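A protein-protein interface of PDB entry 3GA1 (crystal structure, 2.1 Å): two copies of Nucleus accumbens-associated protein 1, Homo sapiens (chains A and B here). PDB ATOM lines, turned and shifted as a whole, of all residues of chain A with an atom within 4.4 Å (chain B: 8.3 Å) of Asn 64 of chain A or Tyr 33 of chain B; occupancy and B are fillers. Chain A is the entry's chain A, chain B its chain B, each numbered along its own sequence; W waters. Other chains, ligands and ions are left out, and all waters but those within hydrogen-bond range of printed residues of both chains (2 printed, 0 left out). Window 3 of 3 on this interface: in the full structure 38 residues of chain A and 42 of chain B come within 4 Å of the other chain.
Position printed for both chains: 35.
Of the 9 pairs that touch across the chains among the printed residues, none has its exchanged pair printed and touching as well.
Water W1 lies within hydrogen-bond range of OD2 of Asp 35 of chain A (2.8 Å), N of Ala 50 of chain A (2.8 Å) and O of Tyr 33 of chain B (2.9 Å).
Water W2 bridges the side-chain hydroxyl of Tyr 33 of chain B (2.8 Å) and the side-chain amide oxygen of Asn 64 of chain A (3.4 Å).
Among the printed residues, pairs that only touch across the chains: Ala 50 of chain A with Leu 24 of chain B (3.7 Å), Ala 50 of chain A with Tyr 33 of chain B (3.9 Å), Ala 50 of chain A with His 48 of chain B (3.4 Å), Ala 53 of chain A with Gln 27 of chain B (3.9 Å), Ala 53 of chain A with Tyr 33 of chain B (3.6 Å) and Phe 63 of chain A with Tyr 33 of chain B (3.8 Å).
Hydrophobic or aromatic side chains of chain B within 4 Å of the printed part of chain A: Leu 24, Tyr 33 and His 48.
Of the 10 printed residues of chain A, 5 touch a printed residue of chain B.
Hydrophobic or aromatic side chains of chain A within 4 Å of the printed part of chain B: Ala 50, Ala 53 and Phe 63.
Among the printed residues, 9 pairs touch across the chains.
O of Arg 60 of chain A sits close to OH of Tyr 33 of chain B (3.2 Å).
O of Ala 50 of chain A is in hydrogen-bond range of NE2 of Gln 27 of chain B (3.1 Å).
OH of Tyr 33 of chain B sits at hydrogen-bond distance from OD1 of Asn 64 of chain A, 2.6 Å away.
O of Arg 60 of chain A lies close to OD1 of Asn 64 of chain A (3.0 Å).
The backbone NH (N) of Leu 32 of chain B is in hydrogen-bond range of the backbone carbonyl oxygen (O) of Gln 27 of chain B, at 2.8 Å.
A ring nitrogen (NE2) of His 48 of chain B lies within hydrogen-bond range of the side-chain amide oxygen (OE1) of Gln 27 of chain B (3.4 Å).
The backbone carbonyl oxygen (O) of Leu 32 of chain B sits at hydrogen-bond distance from a ring nitrogen (NE2) of His 48 of chain B, 3.4 Å away.
The backbone carbonyl oxygen (O) of Ala 53 of chain A sits at hydrogen-bond distance from the guanidinium group (NH2) of Arg 60 of chain A.
The side-chain hydroxyl (OH) of Tyr 90 of chain B sits at hydrogen-bond distance from a ring nitrogen (ND1) of His 48 of chain B (2.5 Å).
Asp 35 of chain A touches none of the printed residues of chain B.
Of the printed residues of chain B, Arg 60 of chain A touches Tyr 33 (2.9 Å).
Of the printed residues of chain B, Phe 63 of chain A touches Tyr 33.
Asn 64 of chain A touches one residue of chain B.
Printed residues of chain A within 4 Å of Tyr 33 of chain B: Ala 50 (3.9 Å), Ala 53 (3.6 Å), Arg 60 (2.9 Å), Phe 63 (3.8 Å) and Asn 64 (2.6 Å).
Printed residues of chain A within 4 Å of His 48 of chain B: Ala 50 (3.4 Å).
The nearest residue of chain B that does not touch Asn 64 of chain A is Leu 32 of chain B (4.7 Å).
The nearest residue of chain A that does not touch Tyr 33 of chain B is Asp 35 of chain A (4.2 Å).
The nearest printed residue of chain B that does not touch Ala 50 of chain A is Leu 32 of chain B (5.4 Å).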
ATOM      1  N   ASP A  35      -6.851   6.687 -26.428  1.00  0.00           N
ATOM      2  CA  ASP A  35      -8.165   6.558 -27.073  1.00  0.00           C
ATOM      3  C   ASP A  35      -9.313   7.031 -26.182  1.00  0.00           C
ATOM      4  O   ASP A  35     -10.474   6.863 -26.538  1.00  0.00           O
ATOM      5  CB  ASP A  35      -8.416   5.121 -27.498  1.00  0.00           C
ATOM      6  CG  ASP A  35      -8.452   4.162 -26.319  1.00  0.00           C
ATOM      7  OD1 ASP A  35      -7.997   4.525 -25.217  1.00  0.00           O
ATOM      8  OD2 ASP A  35      -8.962   3.040 -26.486  1.00  0.00           O
ATOM      9  N   ALA A  50      -7.951   0.413 -22.404  1.00  0.00           N
ATOM     10  CA  ALA A  50      -7.481  -0.904 -22.065  1.00  0.00           C
ATOM     11  C   ALA A  50      -6.830  -0.953 -20.696  1.00  0.00           C
ATOM     12  O   ALA A  50      -7.085  -1.876 -19.906  1.00  0.00           O
ATOM     13  CB  ALA A  50      -6.487  -1.430 -23.157  1.00  0.00           C
ATOM     14  N   ALA A  53      -9.382  -0.272 -17.887  1.00  0.00           N
ATOM     15  CA  ALA A  53     -10.233  -1.440 -17.779  1.00  0.00           C
ATOM     16  C   ALA A  53      -9.540  -2.587 -17.033  1.00  0.00           C
ATOM     17  O   ALA A  53     -10.170  -3.347 -16.293  1.00  0.00           O
ATOM     18  CB  ALA A  53     -10.632  -1.904 -19.173  1.00  0.00           C
ATOM     19  N   ARG A  60     -14.193  -0.886 -16.957  1.00  0.00           N
ATOM     20  CA  ARG A  60     -14.501  -2.053 -17.747  1.00  0.00           C
ATOM     21  C   ARG A  60     -15.959  -2.002 -18.201  1.00  0.00           C
ATOM     22  O   ARG A  60     -16.252  -2.185 -19.383  1.00  0.00           O
ATOM     23  CB  ARG A  60     -14.219  -3.319 -16.936  1.00  0.00           C
ATOM     24  CG  ARG A  60     -14.282  -4.597 -17.709  1.00  0.00           C
ATOM     25  CD  ARG A  60     -13.877  -5.801 -16.831  1.00  0.00           C
ATOM     26  NE  ARG A  60     -12.540  -5.610 -16.288  1.00  0.00           N
ATOM     27  CZ  ARG A  60     -12.259  -5.506 -14.990  1.00  0.00           C
ATOM     28  NH1 ARG A  60     -13.233  -5.610 -14.093  1.00  0.00           N
ATOM     29  NH2 ARG A  60     -11.007  -5.308 -14.586  1.00  0.00           N
ATOM     30  N   ASP A  61     -16.872  -1.745 -17.269  1.00  0.00           N
ATOM     31  CA  ASP A  61     -18.296  -1.757 -17.578  1.00  0.00           C
ATOM     32  C   ASP A  61     -18.682  -0.529 -18.392  1.00  0.00           C
ATOM     33  O   ASP A  61     -19.470  -0.617 -19.315  1.00  0.00           O
ATOM     34  CB  ASP A  61     -19.133  -1.828 -16.294  1.00  0.00           C
ATOM     35  CG  ASP A  61     -19.068  -3.211 -15.629  1.00  0.00           C
ATOM     36  OD1 ASP A  61     -18.442  -4.150 -16.200  1.00  0.00           O
ATOM     37  OD2 ASP A  61     -19.641  -3.366 -14.530  1.00  0.00           O
ATOM     38  N   LEU A  62     -18.122   0.615 -18.048  1.00  0.00           N
ATOM     39  CA  LEU A  62     -18.343   1.834 -18.817  1.00  0.00           C
ATOM     40  C   LEU A  62     -17.884   1.721 -20.294  1.00  0.00           C
ATOM     41  O   LEU A  62     -18.635   2.032 -21.221  1.00  0.00           O
ATOM     42  CB  LEU A  62     -17.589   2.969 -18.143  1.00  0.00           C
ATOM     43  CG  LEU A  62     -17.721   4.276 -18.883  1.00  0.00           C
ATOM     44  CD1 LEU A  62     -19.219   4.580 -18.955  1.00  0.00           C
ATOM     45  CD2 LEU A  62     -16.916   5.375 -18.215  1.00  0.00           C
ATOM     46  N   PHE A  63     -16.652   1.268 -20.503  1.00  0.00           N
ATOM     47  CA  PHE A  63     -16.108   1.146 -21.866  1.00  0.00           C
ATOM     48  C   PHE A  63     -16.742  -0.025 -22.637  1.00  0.00           C
ATOM     49  O   PHE A  63     -16.746  -0.036 -23.862  1.00  0.00           O
ATOM     50  CB  PHE A  63     -14.570   1.090 -21.833  1.00  0.00           C
ATOM     51  CG  PHE A  63     -13.938   2.350 -21.283  1.00  0.00           C
ATOM     52  CD1 PHE A  63     -14.510   3.591 -21.534  1.00  0.00           C
ATOM     53  CD2 PHE A  63     -12.779   2.302 -20.526  1.00  0.00           C
ATOM     54  CE1 PHE A  63     -13.965   4.741 -21.031  1.00  0.00           C
ATOM     55  CE2 PHE A  63     -12.215   3.459 -20.021  1.00  0.00           C
ATOM     56  CZ  PHE A  63     -12.799   4.677 -20.271  1.00  0.00           C
ATOM     57  N   ASN A  64     -17.308  -1.001 -21.928  1.00  0.00           N
ATOM     58  CA  ASN A  64     -18.121  -2.023 -22.573  1.00  0.00           C
ATOM     59  C   ASN A  64     -19.378  -1.419 -23.179  1.00  0.00           C
ATOM     60  O   ASN A  64     -19.979  -1.990 -24.086  1.00  0.00           O
ATOM     61  CB  ASN A  64     -18.612  -3.055 -21.560  1.00  0.00           C
ATOM     62  CG  ASN A  64     -17.544  -4.027 -21.123  1.00  0.00           C
ATOM     63  OD1 ASN A  64     -16.420  -4.060 -21.661  1.00  0.00           O
ATOM     64  ND2 ASN A  64     -17.894  -4.847 -20.121  1.00  0.00           N
ATOM     65  N   ASN A  65     -19.831  -0.296 -22.637  1.00  0.00           N
ATOM     66  CA  ASN A  65     -21.166   0.173 -22.944  1.00  0.00           C
ATOM     67  C   ASN A  65     -21.230   1.573 -23.533  1.00  0.00           C
ATOM     68  O   ASN A  65     -22.314   2.127 -23.725  1.00  0.00           O
ATOM     69  CB  ASN A  65     -22.030   0.065 -21.689  1.00  0.00           C
ATOM     70  CG  ASN A  65     -22.180  -1.396 -21.222  1.00  0.00           C
ATOM     71  OD1 ASN A  65     -21.745  -1.772 -20.126  1.00  0.00           O
ATOM     72  ND2 ASN A  65     -22.752  -2.227 -22.088  1.00  0.00           N
ATOM     73  N   SER A  66     -20.075   2.129 -23.857  1.00  0.00           N
ATOM     74  CA  SER A  66     -20.021   3.444 -24.420  1.00  0.00           C
ATOM     75  C   SER A  66     -18.745   3.593 -25.222  1.00  0.00           C
ATOM     76  O   SER A  66     -17.673   3.126 -24.800  1.00  0.00           O
ATOM     77  CB  SER A  66     -20.041   4.494 -23.321  1.00  0.00           C
ATOM     78  OG  SER A  66     -19.750   5.775 -23.846  1.00  0.00           O
ATOM     79  N   CYS B  23      -3.475  -9.194 -18.853  1.00  0.00           N
ATOM     80  CA  CYS B  23      -4.844  -8.723 -18.914  1.00  0.00           C
ATOM     81  C   CYS B  23      -5.084  -8.123 -20.301  1.00  0.00           C
ATOM     82  O   CYS B  23      -6.099  -8.412 -20.937  1.00  0.00           O
ATOM     83  CB  CYS B  23      -5.151  -7.705 -17.841  1.00  0.00           C
ATOM     84  SG  CYS B  23      -6.885  -7.295 -17.831  1.00  0.00           S
ATOM     85  N   LEU B  24      -4.128  -7.315 -20.773  1.00  0.00           N
ATOM     86  CA  LEU B  24      -4.221  -6.724 -22.098  1.00  0.00           C
ATOM     87  C   LEU B  24      -4.258  -7.805 -23.169  1.00  0.00           C
ATOM     88  O   LEU B  24      -4.970  -7.700 -24.145  1.00  0.00           O
ATOM     89  CB  LEU B  24      -3.047  -5.777 -22.365  1.00  0.00           C
ATOM     90  CG  LEU B  24      -2.918  -4.556 -21.446  1.00  0.00           C
ATOM     91  CD1 LEU B  24      -1.873  -3.557 -21.940  1.00  0.00           C
ATOM     92  CD2 LEU B  24      -4.230  -3.870 -21.267  1.00  0.00           C
ATOM     93  N   GLU B  26      -5.436 -10.883 -22.855  1.00  0.00           N
ATOM     94  CA  GLU B  26      -6.751 -11.514 -22.755  1.00  0.00           C
ATOM     95  C   GLU B  26      -7.808 -10.618 -23.381  1.00  0.00           C
ATOM     96  O   GLU B  26      -8.670 -11.096 -24.083  1.00  0.00           O
ATOM     97  CB  GLU B  26      -7.098 -11.808 -21.283  1.00  0.00           C
ATOM     98  CG  GLU B  26      -6.135 -12.828 -20.641  1.00  0.00           C
ATOM     99  CD  GLU B  26      -6.193 -12.874 -19.095  1.00  0.00           C
ATOM    100  OE1 GLU B  26      -6.900 -12.027 -18.462  1.00  0.00           O
ATOM    101  OE2 GLU B  26      -5.502 -13.762 -18.512  1.00  0.00           O
ATOM    102  N   GLN B  27      -7.737  -9.315 -23.140  1.00  0.00           N
ATOM    103  CA  GLN B  27      -8.679  -8.384 -23.763  1.00  0.00           C
ATOM    104  C   GLN B  27      -8.606  -8.495 -25.290  1.00  0.00           C
ATOM    105  O   GLN B  27      -9.615  -8.622 -25.962  1.00  0.00           O
ATOM    106  CB  GLN B  27      -8.346  -6.960 -23.360  1.00  0.00           C
ATOM    107  CG  GLN B  27      -8.523  -6.603 -21.870  1.00  0.00           C
ATOM    108  CD  GLN B  27      -8.029  -5.173 -21.586  1.00  0.00           C
ATOM    109  OE1 GLN B  27      -7.564  -4.485 -22.501  1.00  0.00           O
ATOM    110  NE2 GLN B  27      -8.158  -4.717 -20.337  1.00  0.00           N
ATOM    111  N   ARG B  28      -7.393  -8.431 -25.834  1.00  0.00           N
ATOM    112  CA  ARG B  28      -7.197  -8.533 -27.278  1.00  0.00           C
ATOM    113  C   ARG B  28      -7.827  -9.818 -27.788  1.00  0.00           C
ATOM    114  O   ARG B  28      -8.615  -9.809 -28.731  1.00  0.00           O
ATOM    115  CB  ARG B  28      -5.708  -8.521 -27.619  1.00  0.00           C
ATOM    116  CG  ARG B  28      -5.407  -9.138 -28.969  1.00  0.00           C
ATOM    117  CD  ARG B  28      -3.927  -9.167 -29.222  1.00  0.00           C
ATOM    118  NE  ARG B  28      -3.256 -10.322 -28.662  1.00  0.00           N
ATOM    119  CZ  ARG B  28      -3.133 -11.490 -29.294  1.00  0.00           C
ATOM    120  NH1 ARG B  28      -3.669 -11.654 -30.491  1.00  0.00           N
ATOM    121  NH2 ARG B  28      -2.467 -12.492 -28.741  1.00  0.00           N
ATOM    122  N   GLN B  30     -10.174 -11.424 -26.802  1.00  0.00           N
ATOM    123  CA  GLN B  30     -11.633 -11.347 -26.809  1.00  0.00           C
ATOM    124  C   GLN B  30     -12.175 -10.163 -27.608  1.00  0.00           C
ATOM    125  O   GLN B  30     -13.367  -9.947 -27.625  1.00  0.00           O
ATOM    126  CB  GLN B  30     -12.180 -11.282 -25.393  1.00  0.00           C
ATOM    127  CG  GLN B  30     -12.259 -12.620 -24.698  1.00  0.00           C
ATOM    128  CD  GLN B  30     -12.300 -12.461 -23.207  1.00  0.00           C
ATOM    129  OE1 GLN B  30     -13.323 -12.076 -22.637  1.00  0.00           O
ATOM    130  NE2 GLN B  30     -11.192 -12.757 -22.555  1.00  0.00           N
ATOM    131  N   GLY B  31     -11.304  -9.415 -28.274  1.00  0.00           N
ATOM    132  CA  GLY B  31     -11.709  -8.209 -29.000  1.00  0.00           C
ATOM    133  C   GLY B  31     -12.158  -7.033 -28.130  1.00  0.00           C
ATOM    134  O   GLY B  31     -13.001  -6.236 -28.556  1.00  0.00           O
ATOM    135  N   LEU B  32     -11.605  -6.888 -26.923  1.00  0.00           N
ATOM    136  CA  LEU B  32     -12.063  -5.818 -26.023  1.00  0.00           C
ATOM    137  C   LEU B  32     -11.118  -4.615 -25.931  1.00  0.00           C
ATOM    138  O   LEU B  32      -9.886  -4.752 -25.773  1.00  0.00           O
ATOM    139  CB  LEU B  32     -12.323  -6.373 -24.626  1.00  0.00           C
ATOM    140  CG  LEU B  32     -13.385  -7.472 -24.531  1.00  0.00           C
ATOM    141  CD1 LEU B  32     -13.402  -8.021 -23.122  1.00  0.00           C
ATOM    142  CD2 LEU B  32     -14.782  -6.983 -24.934  1.00  0.00           C
ATOM    143  N   TYR B  33     -11.716  -3.430 -26.008  1.00  0.00           N
ATOM    144  CA  TYR B  33     -10.988  -2.169 -25.786  1.00  0.00           C
ATOM    145  C   TYR B  33      -9.855  -1.984 -26.810  1.00  0.00           C
ATOM    146  O   TYR B  33      -8.943  -1.203 -26.588  1.00  0.00           O
ATOM    147  CB  TYR B  33     -10.426  -2.113 -24.342  1.00  0.00           C
ATOM    148  CG  TYR B  33     -11.398  -2.625 -23.310  1.00  0.00           C
ATOM    149  CD1 TYR B  33     -12.670  -2.078 -23.186  1.00  0.00           C
ATOM    150  CD2 TYR B  33     -11.068  -3.685 -22.501  1.00  0.00           C
ATOM    151  CE1 TYR B  33     -13.570  -2.572 -22.268  1.00  0.00           C
ATOM    152  CE2 TYR B  33     -11.951  -4.184 -21.583  1.00  0.00           C
ATOM    153  CZ  TYR B  33     -13.198  -3.639 -21.466  1.00  0.00           C
ATOM    154  OH  TYR B  33     -14.059  -4.168 -20.533  1.00  0.00           O
ATOM    155  N   CYS B  34      -9.934  -2.695 -27.927  1.00  0.00           N
ATOM    156  CA  CYS B  34      -8.979  -2.548 -29.022  1.00  0.00           C
ATOM    157  C   CYS B  34      -9.331  -1.339 -29.884  1.00  0.00           C
ATOM    158  O   CYS B  34     -10.510  -1.022 -30.048  1.00  0.00           O
ATOM    159  CB  CYS B  34      -8.978  -3.810 -29.885  1.00  0.00           C
ATOM    160  SG  CYS B  34      -8.302  -5.222 -29.037  1.00  0.00           S
ATOM    161  N   ASP B  35      -8.326  -0.667 -30.436  1.00  0.00           N
ATOM    162  CA  ASP B  35      -8.564   0.576 -31.172  1.00  0.00           C
ATOM    163  C   ASP B  35      -7.978   0.502 -32.585  1.00  0.00           C
ATOM    164  O   ASP B  35      -7.953   1.489 -33.324  1.00  0.00           O
ATOM    165  CB  ASP B  35      -7.968   1.769 -30.412  1.00  0.00           C
ATOM    166  CG  ASP B  35      -6.457   1.640 -30.175  1.00  0.00           C
ATOM    167  OD1 ASP B  35      -5.894   0.547 -30.303  1.00  0.00           O
ATOM    168  OD2 ASP B  35      -5.824   2.646 -29.834  1.00  0.00           O
ATOM    169  N   VAL B  36      -7.515  -0.676 -32.970  1.00  0.00           N
ATOM    170  CA  VAL B  36      -7.065  -0.857 -34.332  1.00  0.00           C
ATOM    171  C   VAL B  36      -7.294  -2.278 -34.763  1.00  0.00           C
ATOM    172  O   VAL B  36      -7.283  -3.199 -33.960  1.00  0.00           O
ATOM    173  CB  VAL B  36      -5.568  -0.506 -34.513  1.00  0.00           C
ATOM    174  CG1 VAL B  36      -4.696  -1.447 -33.707  1.00  0.00           C
ATOM    175  CG2 VAL B  36      -5.184  -0.546 -36.002  1.00  0.00           C
ATOM    176  N   LYS B  46      -7.491  -7.740 -34.157  1.00  0.00           N
ATOM    177  CA  LYS B  46      -7.735  -6.637 -33.248  1.00  0.00           C
ATOM    178  C   LYS B  46      -6.534  -6.481 -32.327  1.00  0.00           C
ATOM    179  O   LYS B  46      -5.896  -7.460 -31.953  1.00  0.00           O
ATOM    180  CB  LYS B  46      -9.002  -6.897 -32.429  1.00  0.00           C
ATOM    181  CG  LYS B  46     -10.267  -7.026 -33.269  1.00  0.00           C
ATOM    182  CD  LYS B  46     -11.420  -7.605 -32.445  1.00  0.00           C
ATOM    183  CE  LYS B  46     -12.729  -7.637 -33.221  1.00  0.00           C
ATOM    184  NZ  LYS B  46     -13.110  -6.264 -33.671  1.00  0.00           N
ATOM    185  N   ALA B  47      -6.225  -5.240 -31.969  1.00  0.00           N
ATOM    186  CA  ALA B  47      -5.071  -4.954 -31.160  1.00  0.00           C
ATOM    187  C   ALA B  47      -5.225  -3.589 -30.517  1.00  0.00           C
ATOM    188  O   ALA B  47      -6.194  -2.870 -30.776  1.00  0.00           O
ATOM    189  CB  ALA B  47      -3.799  -4.993 -32.024  1.00  0.00           C
ATOM    190  N   HIS B  48      -4.257  -3.254 -29.676  1.00  0.00           N
ATOM    191  CA  HIS B  48      -4.146  -1.934 -29.108  1.00  0.00           C
ATOM    192  C   HIS B  48      -2.922  -1.226 -29.701  1.00  0.00           C
ATOM    193  O   HIS B  48      -1.795  -1.676 -29.538  1.00  0.00           O
ATOM    194  CB  HIS B  48      -3.967  -1.999 -27.579  1.00  0.00           C
ATOM    195  CG  HIS B  48      -4.929  -2.910 -26.874  1.00  0.00           C
ATOM    196  ND1 HIS B  48      -4.666  -4.245 -26.650  1.00  0.00           N
ATOM    197  CD2 HIS B  48      -6.129  -2.662 -26.290  1.00  0.00           C
ATOM    198  CE1 HIS B  48      -5.673  -4.785 -25.982  1.00  0.00           C
ATOM    199  NE2 HIS B  48      -6.569  -3.841 -25.739  1.00  0.00           N
ATOM    200  N   ARG B  49      -3.130  -0.080 -30.310  1.00  0.00           N
ATOM    201  CA  ARG B  49      -2.021   0.647 -30.930  1.00  0.00           C
ATOM    202  C   ARG B  49      -0.867   0.854 -29.977  1.00  0.00           C
ATOM    203  O   ARG B  49       0.294   0.746 -30.364  1.00  0.00           O
ATOM    204  CB  ARG B  49      -2.511   1.995 -31.469  1.00  0.00           C
ATOM    205  CG  ARG B  49      -3.452   1.848 -32.640  1.00  0.00           C
ATOM    206  CD  ARG B  49      -4.059   3.187 -33.063  1.00  0.00           C
ATOM    207  NE  ARG B  49      -4.889   3.018 -34.263  1.00  0.00           N
ATOM    208  CZ  ARG B  49      -6.042   3.651 -34.496  1.00  0.00           C
ATOM    209  NH1 ARG B  49      -6.537   4.508 -33.609  1.00  0.00           N
ATOM    210  NH2 ARG B  49      -6.710   3.412 -35.622  1.00  0.00           N
ATOM    211  N   TYR B  90       2.635  -8.914 -26.785  1.00  0.00           N
ATOM    212  CA  TYR B  90       1.739  -8.947 -25.638  1.00  0.00           C
ATOM    213  C   TYR B  90       2.210  -9.915 -24.561  1.00  0.00           C
ATOM    214  O   TYR B  90       1.530 -10.060 -23.559  1.00  0.00           O
ATOM    215  CB  TYR B  90       0.341  -9.389 -26.066  1.00  0.00           C
ATOM    216  CG  TYR B  90      -0.535  -8.289 -26.643  1.00  0.00           C
ATOM    217  CD1 TYR B  90      -0.470  -7.948 -27.987  1.00  0.00           C
ATOM    218  CD2 TYR B  90      -1.441  -7.606 -25.837  1.00  0.00           C
ATOM    219  CE1 TYR B  90      -1.268  -6.946 -28.503  1.00  0.00           C
ATOM    220  CE2 TYR B  90      -2.246  -6.625 -26.348  1.00  0.00           C
ATOM    221  CZ  TYR B  90      -2.161  -6.298 -27.671  1.00  0.00           C
ATOM    222  OH  TYR B  90      -2.983  -5.333 -28.159  1.00  0.00           O
HETATM  223  O   HOH W   1      -7.654   1.004 -25.142  1.00  0.00           O
HETATM  224  O   HOH W   2     -14.982  -6.763 -20.080  1.00  0.00           O
